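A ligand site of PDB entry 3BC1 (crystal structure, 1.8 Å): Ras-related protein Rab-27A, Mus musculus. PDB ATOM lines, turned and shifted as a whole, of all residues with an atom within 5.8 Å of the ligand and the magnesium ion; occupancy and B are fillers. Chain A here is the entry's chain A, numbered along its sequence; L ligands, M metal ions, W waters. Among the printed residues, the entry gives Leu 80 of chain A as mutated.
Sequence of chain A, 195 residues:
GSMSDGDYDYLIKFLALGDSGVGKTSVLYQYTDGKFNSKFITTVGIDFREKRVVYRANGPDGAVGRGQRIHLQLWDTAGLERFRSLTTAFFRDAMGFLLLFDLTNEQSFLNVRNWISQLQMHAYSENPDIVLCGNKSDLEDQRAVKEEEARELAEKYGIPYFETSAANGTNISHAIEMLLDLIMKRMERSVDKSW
The backbone NH of Thr 43 lies close to an oxygen (O3) of the ligand (3.0 Å).
An oxygen (O7) of the ligand lies within hydrogen-bond range of the backbone NH (N) of Thr 25, at 3.4 Å.
An oxygen (O2) of the ligand lies within hydrogen-bond range of the side-chain hydroxyl of Ser 20.
An oxygen (O4) of the ligand is in hydrogen-bond range of the backbone NH of Lys 24 (3.0 Å).
An oxygen (O1) of the ligand lies within salt-bridge range of the side-chain amino group (NZ) of Lys 24, 2.7 Å away.
An oxygen (O2) of the ligand lies within hydrogen-bond range of the side-chain hydroxyl (OG1) of Thr 42 (2.7 Å).
An oxygen (O13) of the ligand is in hydrogen-bond range of the backbone NH (N) of Ala 166, 2.8 Å away.
The side-chain carboxylate (OD1) of Asp 138 lies within hydrogen-bond range of a nitrogen (N4) of the ligand, 2.8 Å away.
O of Asn 37 sits at hydrogen-bond distance from O12 of the ligand (2.8 Å).
The backbone NH of Ser 26 lies within hydrogen-bond range of an oxygen (O7) of the ligand (2.9 Å).
OG of Ser 26 lies within hydrogen-bond range of O7 of the ligand, 2.8 Å away.
The backbone carbonyl oxygen (O) of Ser 38 lies within hydrogen-bond range of an oxygen (O11) of the ligand, at 2.8 Å.
N of Gly 79 lies within hydrogen-bond range of O1 of the ligand (3.0 Å).
The backbone NH (N) of Gly 23 lies within hydrogen-bond range of an oxygen (O4) of the ligand.
ND2 of Asn 135 lies within hydrogen-bond range of N3 of the ligand.
N of Lys 136 sits close to O13 of the ligand (3.4 Å).
O10 of the ligand sits at hydrogen-bond distance from NZ of Lys 136 (3.2 Å).
N of Phe 40 sits at hydrogen-bond distance from O11 of the ligand.
The backbone NH of Val 22 is in hydrogen-bond range of an oxygen (O4) of the ligand (3.4 Å).
N of Ala 167 lies within hydrogen-bond range of O13 of the ligand (3.5 Å).
The side-chain hydroxyl of Thr 25 sits close to the side-chain carboxylate of Asp 76 (2.7 Å).
The backbone carbonyl oxygen (O) of Asp 19 is in hydrogen-bond range of the side-chain amino group (NZ) of Lys 24 (2.7 Å).
OD1 of Asn 37 lies within hydrogen-bond range of N of Lys 39 (3.0 Å).
The side-chain amide nitrogen (ND2) of Asn 135 lies within hydrogen-bond range of the backbone carbonyl oxygen (O) of Val 22, 3.0 Å away.
OD1 of Asn 135 is in hydrogen-bond range of OG1 of Thr 164 (2.9 Å).
NZ of Lys 136 lies within hydrogen-bond range of O of Gly 21, at 2.8 Å.
N of Lys 136 lies within hydrogen-bond range of O of Thr 164 (3.0 Å).
The backbone NH (N) of Asn 168 lies within hydrogen-bond range of the side-chain hydroxyl (OG) of Ser 165 (3.3 Å).
The backbone NH (N) of Gly 21 lies close to a nitrogen (N1) of the ligand, at 3.1 Å.
Residues that only touch the ligand: Phe 36, Ser 165, Leu 139, Lys 39, Ala 78 and Asp 19.
Hydrophobic or aromatic side chains within 4 Å of the ligand: Val 22, Phe 36, Phe 40, Leu 139, Ala 166 and Ala 167.
The nearest printed residue that does not touch the magnesium ion is Asp 76 (4.1 Å).
The magnesium ion is bound by O3 of the ligand (2.0 Å), OG1 of Thr 43 (2.0 Å), OG1 of Thr 25 (2.1 Å), O5 of the ligand (2.1 Å), water W3 (2.1 Å) and water W4 (2.2 Å).
Water W4 bridges O of Ile 41 and O8 of the ligand.
Water W3 bridges OD1 of Asp 76 and O of Thr 77.
Water W1 lies within hydrogen-bond range of an oxygen (O8) of the ligand (2.6 Å), the backbone NH (N) of Ile 41 (2.8 Å) and the backbone carbonyl oxygen (O) of Lys 39 (3.2 Å).
Water W2 lies within hydrogen-bond range of an oxygen (O2) of the ligand, the backbone NH (N) of Leu 80, the backbone NH (N) of Gly 79 and the side-chain hydroxyl (OG1) of Thr 42.
Water W5 lies within hydrogen-bond range of the side-chain amino group of Lys 136 and an oxygen (O10) of the ligand.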
ATOM      1  N   GLY A  18      16.285  16.044  -5.991  1.00  0.00           N
ATOM      2  CA  GLY A  18      16.831  16.398  -4.693  1.00  0.00           C
ATOM      3  C   GLY A  18      15.766  16.316  -3.629  1.00  0.00           C
ATOM      4  O   GLY A  18      14.584  16.137  -3.942  1.00  0.00           O
ATOM      5  N   ASP A  19      16.174  16.444  -2.368  1.00  0.00           N
ATOM      6  CA  ASP A  19      15.264  16.307  -1.241  1.00  0.00           C
ATOM      7  C   ASP A  19      14.171  17.372  -1.277  1.00  0.00           C
ATOM      8  O   ASP A  19      14.338  18.434  -1.889  1.00  0.00           O
ATOM      9  CB  ASP A  19      16.018  16.442   0.091  1.00  0.00           C
ATOM     10  CG  ASP A  19      16.833  15.217   0.441  1.00  0.00           C
ATOM     11  OD1 ASP A  19      16.856  14.223  -0.325  1.00  0.00           O
ATOM     12  OD2 ASP A  19      17.478  15.243   1.512  1.00  0.00           O
ATOM     13  N   SER A  20      13.052  17.102  -0.598  1.00  0.00           N
ATOM     14  CA  SER A  20      11.984  18.085  -0.447  1.00  0.00           C
ATOM     15  C   SER A  20      12.539  19.327   0.239  1.00  0.00           C
ATOM     16  O   SER A  20      13.275  19.233   1.213  1.00  0.00           O
ATOM     17  CB  SER A  20      10.814  17.523   0.366  1.00  0.00           C
ATOM     18  OG  SER A  20       9.760  18.471   0.430  1.00  0.00           O
ATOM     19  N   GLY A  21      12.196  20.497  -0.319  1.00  0.00           N
ATOM     20  CA  GLY A  21      12.537  21.776   0.292  1.00  0.00           C
ATOM     21  C   GLY A  21      13.839  22.421  -0.157  1.00  0.00           C
ATOM     22  O   GLY A  21      14.109  23.559   0.197  1.00  0.00           O
ATOM     23  N   VAL A  22      14.666  21.698  -0.919  1.00  0.00           N
ATOM     24  CA  VAL A  22      15.998  22.203  -1.308  1.00  0.00           C
ATOM     25  C   VAL A  22      15.953  23.367  -2.289  1.00  0.00           C
ATOM     26  O   VAL A  22      16.896  24.169  -2.347  1.00  0.00           O
ATOM     27  CB  VAL A  22      16.897  21.085  -1.902  1.00  0.00           C
ATOM     28  CG1 VAL A  22      17.103  19.966  -0.884  1.00  0.00           C
ATOM     29  CG2 VAL A  22      16.335  20.562  -3.212  1.00  0.00           C
ATOM     30  N   GLY A  23      14.873  23.468  -3.063  1.00  0.00           N
ATOM     31  CA  GLY A  23      14.662  24.613  -3.973  1.00  0.00           C
ATOM     32  C   GLY A  23      14.561  24.289  -5.456  1.00  0.00           C
ATOM     33  O   GLY A  23      14.824  25.143  -6.301  1.00  0.00           O
ATOM     34  N   LYS A  24      14.165  23.057  -5.792  1.00  0.00           N
ATOM     35  CA  LYS A  24      14.083  22.626  -7.187  1.00  0.00           C
ATOM     36  C   LYS A  24      13.079  23.464  -7.988  1.00  0.00           C
ATOM     37  O   LYS A  24      13.381  23.953  -9.081  1.00  0.00           O
ATOM     38  CB  LYS A  24      13.690  21.147  -7.269  1.00  0.00           C
ATOM     39  CG  LYS A  24      14.676  20.224  -6.555  1.00  0.00           C
ATOM     40  CD  LYS A  24      14.185  18.777  -6.503  1.00  0.00           C
ATOM     41  CE  LYS A  24      12.912  18.591  -5.707  1.00  0.00           C
ATOM     42  NZ  LYS A  24      13.074  18.840  -4.276  1.00  0.00           N
ATOM     43  N   THR A  25      11.888  23.643  -7.428  1.00  0.00           N
ATOM     44  CA  THR A  25      10.851  24.431  -8.078  1.00  0.00           C
ATOM     45  C   THR A  25      11.289  25.885  -8.233  1.00  0.00           C
ATOM     46  O   THR A  25      11.153  26.466  -9.308  1.00  0.00           O
ATOM     47  CB  THR A  25       9.525  24.367  -7.302  1.00  0.00           C
ATOM     48  OG1 THR A  25       9.078  23.009  -7.232  1.00  0.00           O
ATOM     49  CG2 THR A  25       8.474  25.224  -7.976  1.00  0.00           C
ATOM     50  N   SER A  26      11.828  26.457  -7.159  1.00  0.00           N
ATOM     51  CA  SER A  26      12.282  27.850  -7.139  1.00  0.00           C
ATOM     52  C   SER A  26      13.401  28.112  -8.150  1.00  0.00           C
ATOM     53  O   SER A  26      13.392  29.106  -8.879  1.00  0.00           O
ATOM     54  CB  SER A  26      12.713  28.265  -5.732  1.00  0.00           C
ATOM     55  OG  SER A  26      11.636  28.136  -4.807  1.00  0.00           O
ATOM     56  N   VAL A  27      14.376  27.210  -8.190  1.00  0.00           N
ATOM     57  CA  VAL A  27      15.474  27.326  -9.143  1.00  0.00           C
ATOM     58  C   VAL A  27      14.935  27.387 -10.564  1.00  0.00           C
ATOM     59  O   VAL A  27      15.286  28.302 -11.317  1.00  0.00           O
ATOM     60  CB  VAL A  27      16.465  26.152  -8.997  1.00  0.00           C
ATOM     61  CG1 VAL A  27      17.361  26.053 -10.231  1.00  0.00           C
ATOM     62  CG2 VAL A  27      17.295  26.330  -7.722  1.00  0.00           C
ATOM     63  N   PHE A  36      10.454  34.700  -8.028  1.00  0.00           N
ATOM     64  CA  PHE A  36      10.662  33.891  -6.825  1.00  0.00           C
ATOM     65  C   PHE A  36       9.504  34.081  -5.833  1.00  0.00           C
ATOM     66  O   PHE A  36       9.069  35.208  -5.602  1.00  0.00           O
ATOM     67  CB  PHE A  36      11.993  34.281  -6.184  1.00  0.00           C
ATOM     68  CG  PHE A  36      12.260  33.617  -4.866  1.00  0.00           C
ATOM     69  CD1 PHE A  36      12.616  32.269  -4.799  1.00  0.00           C
ATOM     70  CD2 PHE A  36      12.188  34.335  -3.677  1.00  0.00           C
ATOM     71  CE1 PHE A  36      12.872  31.650  -3.585  1.00  0.00           C
ATOM     72  CE2 PHE A  36      12.454  33.725  -2.463  1.00  0.00           C
ATOM     73  CZ  PHE A  36      12.791  32.388  -2.407  1.00  0.00           C
ATOM     74  N   ASN A  37       9.027  32.972  -5.268  1.00  0.00           N
ATOM     75  CA  ASN A  37       7.988  32.998  -4.218  1.00  0.00           C
ATOM     76  C   ASN A  37       8.563  32.469  -2.899  1.00  0.00           C
ATOM     77  O   ASN A  37       9.122  31.371  -2.854  1.00  0.00           O
ATOM     78  CB  ASN A  37       6.772  32.154  -4.626  1.00  0.00           C
ATOM     79  CG  ASN A  37       5.569  32.352  -3.697  1.00  0.00           C
ATOM     80  OD1 ASN A  37       5.710  32.836  -2.572  1.00  0.00           O
ATOM     81  ND2 ASN A  37       4.397  31.954  -4.167  1.00  0.00           N
ATOM     82  N   SER A  38       8.431  33.264  -1.838  1.00  0.00           N
ATOM     83  CA  SER A  38       8.964  32.927  -0.523  1.00  0.00           C
ATOM     84  C   SER A  38       8.197  31.808   0.176  1.00  0.00           C
ATOM     85  O   SER A  38       8.753  31.104   1.022  1.00  0.00           O
ATOM     86  CB  SER A  38       8.944  34.179   0.379  1.00  0.00           C
ATOM     87  OG  SER A  38       9.748  35.203  -0.172  1.00  0.00           O
ATOM     88  N   LYS A  39       6.917  31.643  -0.154  1.00  0.00           N
ATOM     89  CA  LYS A  39       6.068  30.657   0.503  1.00  0.00           C
ATOM     90  C   LYS A  39       6.351  29.270  -0.054  1.00  0.00           C
ATOM     91  O   LYS A  39       6.360  29.084  -1.278  1.00  0.00           O
ATOM     92  CB  LYS A  39       4.591  31.000   0.313  1.00  0.00           C
ATOM     93  CG  LYS A  39       3.637  30.096   1.109  1.00  0.00           C
ATOM     94  CD  LYS A  39       2.186  30.443   0.820  1.00  0.00           C
ATOM     95  CE  LYS A  39       1.232  29.374   1.334  1.00  0.00           C
ATOM     96  NZ  LYS A  39      -0.182  29.805   1.174  1.00  0.00           N
ATOM     97  N   PHE A  40       6.561  28.304   0.836  1.00  0.00           N
ATOM     98  CA  PHE A  40       6.794  26.918   0.436  1.00  0.00           C
ATOM     99  C   PHE A  40       5.514  26.281  -0.088  1.00  0.00           C
ATOM    100  O   PHE A  40       4.581  26.016   0.673  1.00  0.00           O
ATOM    101  CB  PHE A  40       7.334  26.133   1.637  1.00  0.00           C
ATOM    102  CG  PHE A  40       7.760  24.713   1.331  1.00  0.00           C
ATOM    103  CD1 PHE A  40       7.982  24.262   0.036  1.00  0.00           C
ATOM    104  CD2 PHE A  40       7.984  23.815   2.379  1.00  0.00           C
ATOM    105  CE1 PHE A  40       8.380  22.956  -0.208  1.00  0.00           C
ATOM    106  CE2 PHE A  40       8.392  22.508   2.126  1.00  0.00           C
ATOM    107  CZ  PHE A  40       8.585  22.089   0.837  1.00  0.00           C
ATOM    108  N   ILE A  41       5.467  26.063  -1.403  1.00  0.00           N
ATOM    109  CA  ILE A  41       4.381  25.320  -2.039  1.00  0.00           C
ATOM    110  C   ILE A  41       4.979  24.028  -2.602  1.00  0.00           C
ATOM    111  O   ILE A  41       5.568  24.012  -3.679  1.00  0.00           O
ATOM    112  CB  ILE A  41       3.676  26.127  -3.161  1.00  0.00           C
ATOM    113  CG1 ILE A  41       3.247  27.518  -2.663  1.00  0.00           C
ATOM    114  CG2 ILE A  41       2.459  25.379  -3.644  1.00  0.00           C
ATOM    115  CD1 ILE A  41       2.820  28.461  -3.796  1.00  0.00           C
ATOM    116  N   THR A  42       4.831  22.943  -1.838  1.00  0.00           N
ATOM    117  CA  THR A  42       5.457  21.671  -2.180  1.00  0.00           C
ATOM    118  C   THR A  42       4.838  21.082  -3.448  1.00  0.00           C
ATOM    119  O   THR A  42       3.637  21.217  -3.700  1.00  0.00           O
ATOM    120  CB  THR A  42       5.407  20.663  -1.002  1.00  0.00           C
ATOM    121  OG1 THR A  42       6.284  19.554  -1.248  1.00  0.00           O
ATOM    122  CG2 THR A  42       3.974  20.175  -0.751  1.00  0.00           C
ATOM    123  N   THR A  43       5.683  20.446  -4.254  1.00  0.00           N
ATOM    124  CA  THR A  43       5.284  19.995  -5.568  1.00  0.00           C
ATOM    125  C   THR A  43       4.456  18.718  -5.446  1.00  0.00           C
ATOM    126  O   THR A  43       4.840  17.774  -4.747  1.00  0.00           O
ATOM    127  CB  THR A  43       6.515  19.755  -6.483  1.00  0.00           C
ATOM    128  OG1 THR A  43       7.215  20.994  -6.670  1.00  0.00           O
ATOM    129  CG2 THR A  43       6.103  19.182  -7.830  1.00  0.00           C
ATOM    130  N   ASP A  76      10.343  19.013 -13.132  1.00  0.00           N
ATOM    131  CA  ASP A  76      10.423  19.393 -11.754  1.00  0.00           C
ATOM    132  C   ASP A  76       9.808  18.295 -10.906  1.00  0.00           C
ATOM    133  O   ASP A  76       8.575  18.147 -10.863  1.00  0.00           O
ATOM    134  CB  ASP A  76       9.669  20.714 -11.563  1.00  0.00           C
ATOM    135  CG  ASP A  76       9.767  21.264 -10.173  1.00  0.00           C
ATOM    136  OD1 ASP A  76      10.629  20.792  -9.402  1.00  0.00           O
ATOM    137  OD2 ASP A  76       8.965  22.183  -9.842  1.00  0.00           O
ATOM    138  N   THR A  77      10.652  17.508 -10.229  1.00  0.00           N
ATOM    139  CA  THR A  77      10.180  16.359  -9.460  1.00  0.00           C
ATOM    140  C   THR A  77       9.963  16.718  -7.999  1.00  0.00           C
ATOM    141  O   THR A  77      10.659  17.565  -7.452  1.00  0.00           O
ATOM    142  CB  THR A  77      11.164  15.163  -9.544  1.00  0.00           C
ATOM    143  OG1 THR A  77      12.437  15.502  -8.974  1.00  0.00           O
ATOM    144  CG2 THR A  77      11.335  14.697 -10.992  1.00  0.00           C
ATOM    145  N   ALA A  78       9.009  16.047  -7.357  1.00  0.00           N
ATOM    146  CA  ALA A  78       8.813  16.184  -5.911  1.00  0.00           C
ATOM    147  C   ALA A  78       9.862  15.371  -5.149  1.00  0.00           C
ATOM    148  O   ALA A  78      10.252  14.285  -5.596  1.00  0.00           O
ATOM    149  CB  ALA A  78       7.404  15.743  -5.511  1.00  0.00           C
ATOM    150  N   GLY A  79      10.306  15.901  -4.018  1.00  0.00           N
ATOM    151  CA  GLY A  79      11.339  15.282  -3.198  1.00  0.00           C
ATOM    152  C   GLY A  79      10.826  14.311  -2.141  1.00  0.00           C
ATOM    153  O   GLY A  79      11.571  13.457  -1.687  1.00  0.00           O
ATOM    154  N   LEU A  80       9.564  14.454  -1.744  1.00  0.00           N
ATOM    155  CA  LEU A  80       8.998  13.584  -0.717  1.00  0.00           C
ATOM    156  C   LEU A  80       8.874  12.140  -1.225  1.00  0.00           C
ATOM    157  O   LEU A  80       8.464  11.909  -2.360  1.00  0.00           O
ATOM    158  CB  LEU A  80       7.628  14.086  -0.266  1.00  0.00           C
ATOM    159  CG  LEU A  80       7.595  15.375   0.552  1.00  0.00           C
ATOM    160  CD1 LEU A  80       6.149  15.656   0.930  1.00  0.00           C
ATOM    161  CD2 LEU A  80       8.476  15.277   1.775  1.00  0.00           C
ATOM    162  N   ASN A 135      22.057  24.939  -3.301  1.00  0.00           N
ATOM    163  CA  ASN A 135      21.118  26.054  -3.360  1.00  0.00           C
ATOM    164  C   ASN A 135      20.938  26.806  -2.029  1.00  0.00           C
ATOM    165  O   ASN A 135      21.340  26.321  -0.974  1.00  0.00           O
ATOM    166  CB  ASN A 135      19.766  25.561  -3.896  1.00  0.00           C
ATOM    167  CG  ASN A 135      18.842  26.696  -4.328  1.00  0.00           C
ATOM    168  OD1 ASN A 135      19.250  27.630  -5.038  1.00  0.00           O
ATOM    169  ND2 ASN A 135      17.597  26.630  -3.888  1.00  0.00           N
ATOM    170  N   LYS A 136      20.336  27.993  -2.122  1.00  0.00           N
ATOM    171  CA  LYS A 136      20.085  28.908  -0.995  1.00  0.00           C
ATOM    172  C   LYS A 136      21.370  29.582  -0.523  1.00  0.00           C
ATOM    173  O   LYS A 136      21.565  29.807   0.680  1.00  0.00           O
ATOM    174  CB  LYS A 136      19.348  28.193   0.154  1.00  0.00           C
ATOM    175  CG  LYS A 136      18.155  27.366  -0.293  1.00  0.00           C
ATOM    176  CD  LYS A 136      17.142  27.154   0.821  1.00  0.00           C
ATOM    177  CE  LYS A 136      16.043  26.191   0.377  1.00  0.00           C
ATOM    178  NZ  LYS A 136      15.150  25.773   1.500  1.00  0.00           N
ATOM    179  N   SER A 137      22.229  29.940  -1.474  1.00  0.00           N
ATOM    180  CA  SER A 137      23.511  30.577  -1.141  1.00  0.00           C
ATOM    181  C   SER A 137      23.333  31.964  -0.498  1.00  0.00           C
ATOM    182  O   SER A 137      24.212  32.440   0.221  1.00  0.00           O
ATOM    183  CB  SER A 137      24.435  30.667  -2.365  1.00  0.00           C
ATOM    184  OG  SER A 137      23.884  31.462  -3.386  1.00  0.00           O
ATOM    185  N   ASP A 138      22.173  32.589  -0.744  1.00  0.00           N
ATOM    186  CA  ASP A 138      21.851  33.871  -0.123  1.00  0.00           C
ATOM    187  C   ASP A 138      21.631  33.793   1.403  1.00  0.00           C
ATOM    188  O   ASP A 138      21.625  34.822   2.077  1.00  0.00           O
ATOM    189  CB  ASP A 138      20.619  34.528  -0.787  1.00  0.00           C
ATOM    190  CG  ASP A 138      19.370  33.661  -0.694  1.00  0.00           C
ATOM    191  OD1 ASP A 138      19.378  32.567  -1.284  1.00  0.00           O
ATOM    192  OD2 ASP A 138      18.395  34.085  -0.034  1.00  0.00           O
ATOM    193  N   LEU A 139      21.461  32.577   1.943  1.00  0.00           N
ATOM    194  CA  LEU A 139      21.182  32.406   3.370  1.00  0.00           C
ATOM    195  C   LEU A 139      22.459  32.034   4.151  1.00  0.00           C
ATOM    196  O   LEU A 139      22.478  31.050   4.890  1.00  0.00           O
ATOM    197  CB  LEU A 139      20.107  31.336   3.576  1.00  0.00           C
ATOM    198  CG  LEU A 139      18.712  31.646   3.022  1.00  0.00           C
ATOM    199  CD1 LEU A 139      17.744  30.541   3.407  1.00  0.00           C
ATOM    200  CD2 LEU A 139      18.200  33.001   3.527  1.00  0.00           C
ATOM    201  N   THR A 164      24.119  28.172  -5.826  1.00  0.00           N
ATOM    202  CA  THR A 164      23.050  28.902  -6.474  1.00  0.00           C
ATOM    203  C   THR A 164      22.124  29.573  -5.464  1.00  0.00           C
ATOM    204  O   THR A 164      22.093  29.216  -4.282  1.00  0.00           O
ATOM    205  CB  THR A 164      22.181  27.975  -7.357  1.00  0.00           C
ATOM    206  OG1 THR A 164      21.593  26.964  -6.553  1.00  0.00           O
ATOM    207  CG2 THR A 164      23.014  27.324  -8.454  1.00  0.00           C
ATOM    208  N   SER A 165      21.388  30.565  -5.956  1.00  0.00           N
ATOM    209  CA  SER A 165      20.275  31.150  -5.224  1.00  0.00           C
ATOM    210  C   SER A 165      19.099  31.328  -6.158  1.00  0.00           C
ATOM    211  O   SER A 165      19.184  32.095  -7.109  1.00  0.00           O
ATOM    212  CB  SER A 165      20.651  32.516  -4.635  1.00  0.00           C
ATOM    213  OG  SER A 165      19.518  33.124  -4.046  1.00  0.00           O
ATOM    214  N   ALA A 166      18.016  30.603  -5.892  1.00  0.00           N
ATOM    215  CA  ALA A 166      16.755  30.808  -6.592  1.00  0.00           C
ATOM    216  C   ALA A 166      16.109  32.144  -6.195  1.00  0.00           C
ATOM    217  O   ALA A 166      15.266  32.668  -6.918  1.00  0.00           O
ATOM    218  CB  ALA A 166      15.793  29.646  -6.325  1.00  0.00           C
ATOM    219  N   ALA A 167      16.502  32.688  -5.038  1.00  0.00           N
ATOM    220  CA  ALA A 167      15.980  33.981  -4.580  1.00  0.00           C
ATOM    221  C   ALA A 167      16.402  35.114  -5.512  1.00  0.00           C
ATOM    222  O   ALA A 167      15.573  35.892  -5.967  1.00  0.00           O
ATOM    223  CB  ALA A 167      16.444  34.265  -3.153  1.00  0.00           C
ATOM    224  N   ASN A 168      17.698  35.185  -5.808  1.00  0.00           N
ATOM    225  CA  ASN A 168      18.230  36.300  -6.601  1.00  0.00           C
ATOM    226  C   ASN A 168      18.809  35.888  -7.968  1.00  0.00           C
ATOM    227  O   ASN A 168      19.209  36.749  -8.744  1.00  0.00           O
ATOM    228  CB  ASN A 168      19.247  37.096  -5.781  1.00  0.00           C
ATOM    229  CG  ASN A 168      20.470  36.274  -5.400  1.00  0.00           C
ATOM    230  OD1 ASN A 168      20.931  35.429  -6.167  1.00  0.00           O
ATOM    231  ND2 ASN A 168      21.010  36.551  -4.229  1.00  0.00           N
HETATM  232  P1  LIG L   1       9.577  19.906  -3.094  1.00  0.00           P
HETATM  233  O1  LIG L   1      10.497  18.859  -3.651  1.00  0.00           O
HETATM  234  O2  LIG L   1       8.906  19.537  -1.800  1.00  0.00           O
HETATM  235  O3  LIG L   1       8.654  20.333  -4.208  1.00  0.00           O
HETATM  236  N1  LIG L   1      10.406  21.229  -2.717  1.00  0.00           N
HETATM  237  P2  LIG L   1      11.367  22.053  -3.678  1.00  0.00           P
HETATM  238  O4  LIG L   1      12.738  21.472  -3.732  1.00  0.00           O
HETATM  239  O5  LIG L   1      10.677  22.331  -4.940  1.00  0.00           O
HETATM  240  O6  LIG L   1      11.573  23.405  -2.949  1.00  0.00           O
HETATM  241  P3  LIG L   1      10.922  24.785  -3.247  1.00  0.00           P
HETATM  242  O7  LIG L   1      11.469  25.332  -4.519  1.00  0.00           O
HETATM  243  O8  LIG L   1       9.463  24.717  -3.051  1.00  0.00           O
HETATM  244  O9  LIG L   1      11.497  25.759  -2.123  1.00  0.00           O
HETATM  245  C1  LIG L   1      11.345  25.450  -0.730  1.00  0.00           C
HETATM  246  C2  LIG L   1      11.367  26.709   0.144  1.00  0.00           C
HETATM  247  O10 LIG L   1      12.680  27.304   0.110  1.00  0.00           O
HETATM  248  C3  LIG L   1      10.421  27.836  -0.268  1.00  0.00           C
HETATM  249  O11 LIG L   1       9.928  28.523   0.888  1.00  0.00           O
HETATM  250  C4  LIG L   1      11.290  28.729  -1.138  1.00  0.00           C
HETATM  251  O12 LIG L   1      10.888  30.084  -1.109  1.00  0.00           O
HETATM  252  C5  LIG L   1      12.645  28.599  -0.457  1.00  0.00           C
HETATM  253  N2  LIG L   1      13.810  28.736  -1.327  1.00  0.00           N
HETATM  254  C6  LIG L   1      14.126  27.980  -2.429  1.00  0.00           C
HETATM  255  N3  LIG L   1      15.251  28.336  -2.993  1.00  0.00           N
HETATM  256  C7  LIG L   1      15.721  29.388  -2.210  1.00  0.00           C
HETATM  257  C8  LIG L   1      16.906  30.156  -2.322  1.00  0.00           C
HETATM  258  O13 LIG L   1      17.799  30.056  -3.185  1.00  0.00           O
HETATM  259  N4  LIG L   1      16.998  31.137  -1.318  1.00  0.00           N
HETATM  260  C9  LIG L   1      16.059  31.297  -0.321  1.00  0.00           C
HETATM  261  N5  LIG L   1      16.278  32.276   0.571  1.00  0.00           N
HETATM  262  N6  LIG L   1      14.945  30.576  -0.197  1.00  0.00           N
HETATM  263  C10 LIG L   1      14.845  29.646  -1.185  1.00  0.00           C
HETATM  264 MG    MG M   1       8.900  21.624  -5.730  1.00  0.00          MG
HETATM  265  O   HOH W   1       7.725  26.666  -2.875  1.00  0.00           O
HETATM  266  O   HOH W   2       7.958  16.928  -2.323  1.00  0.00           O
HETATM  267  O   HOH W   3       9.979  20.229  -6.831  1.00  0.00           O
HETATM  268  O   HOH W   4       7.891  23.235  -4.638  1.00  0.00           O
HETATM  269  O   HOH W   5      14.474  27.982   3.001  1.00  0.00           O
HETATM  270  O   HOH W   6      13.830  32.949   2.481  1.00  0.00           O
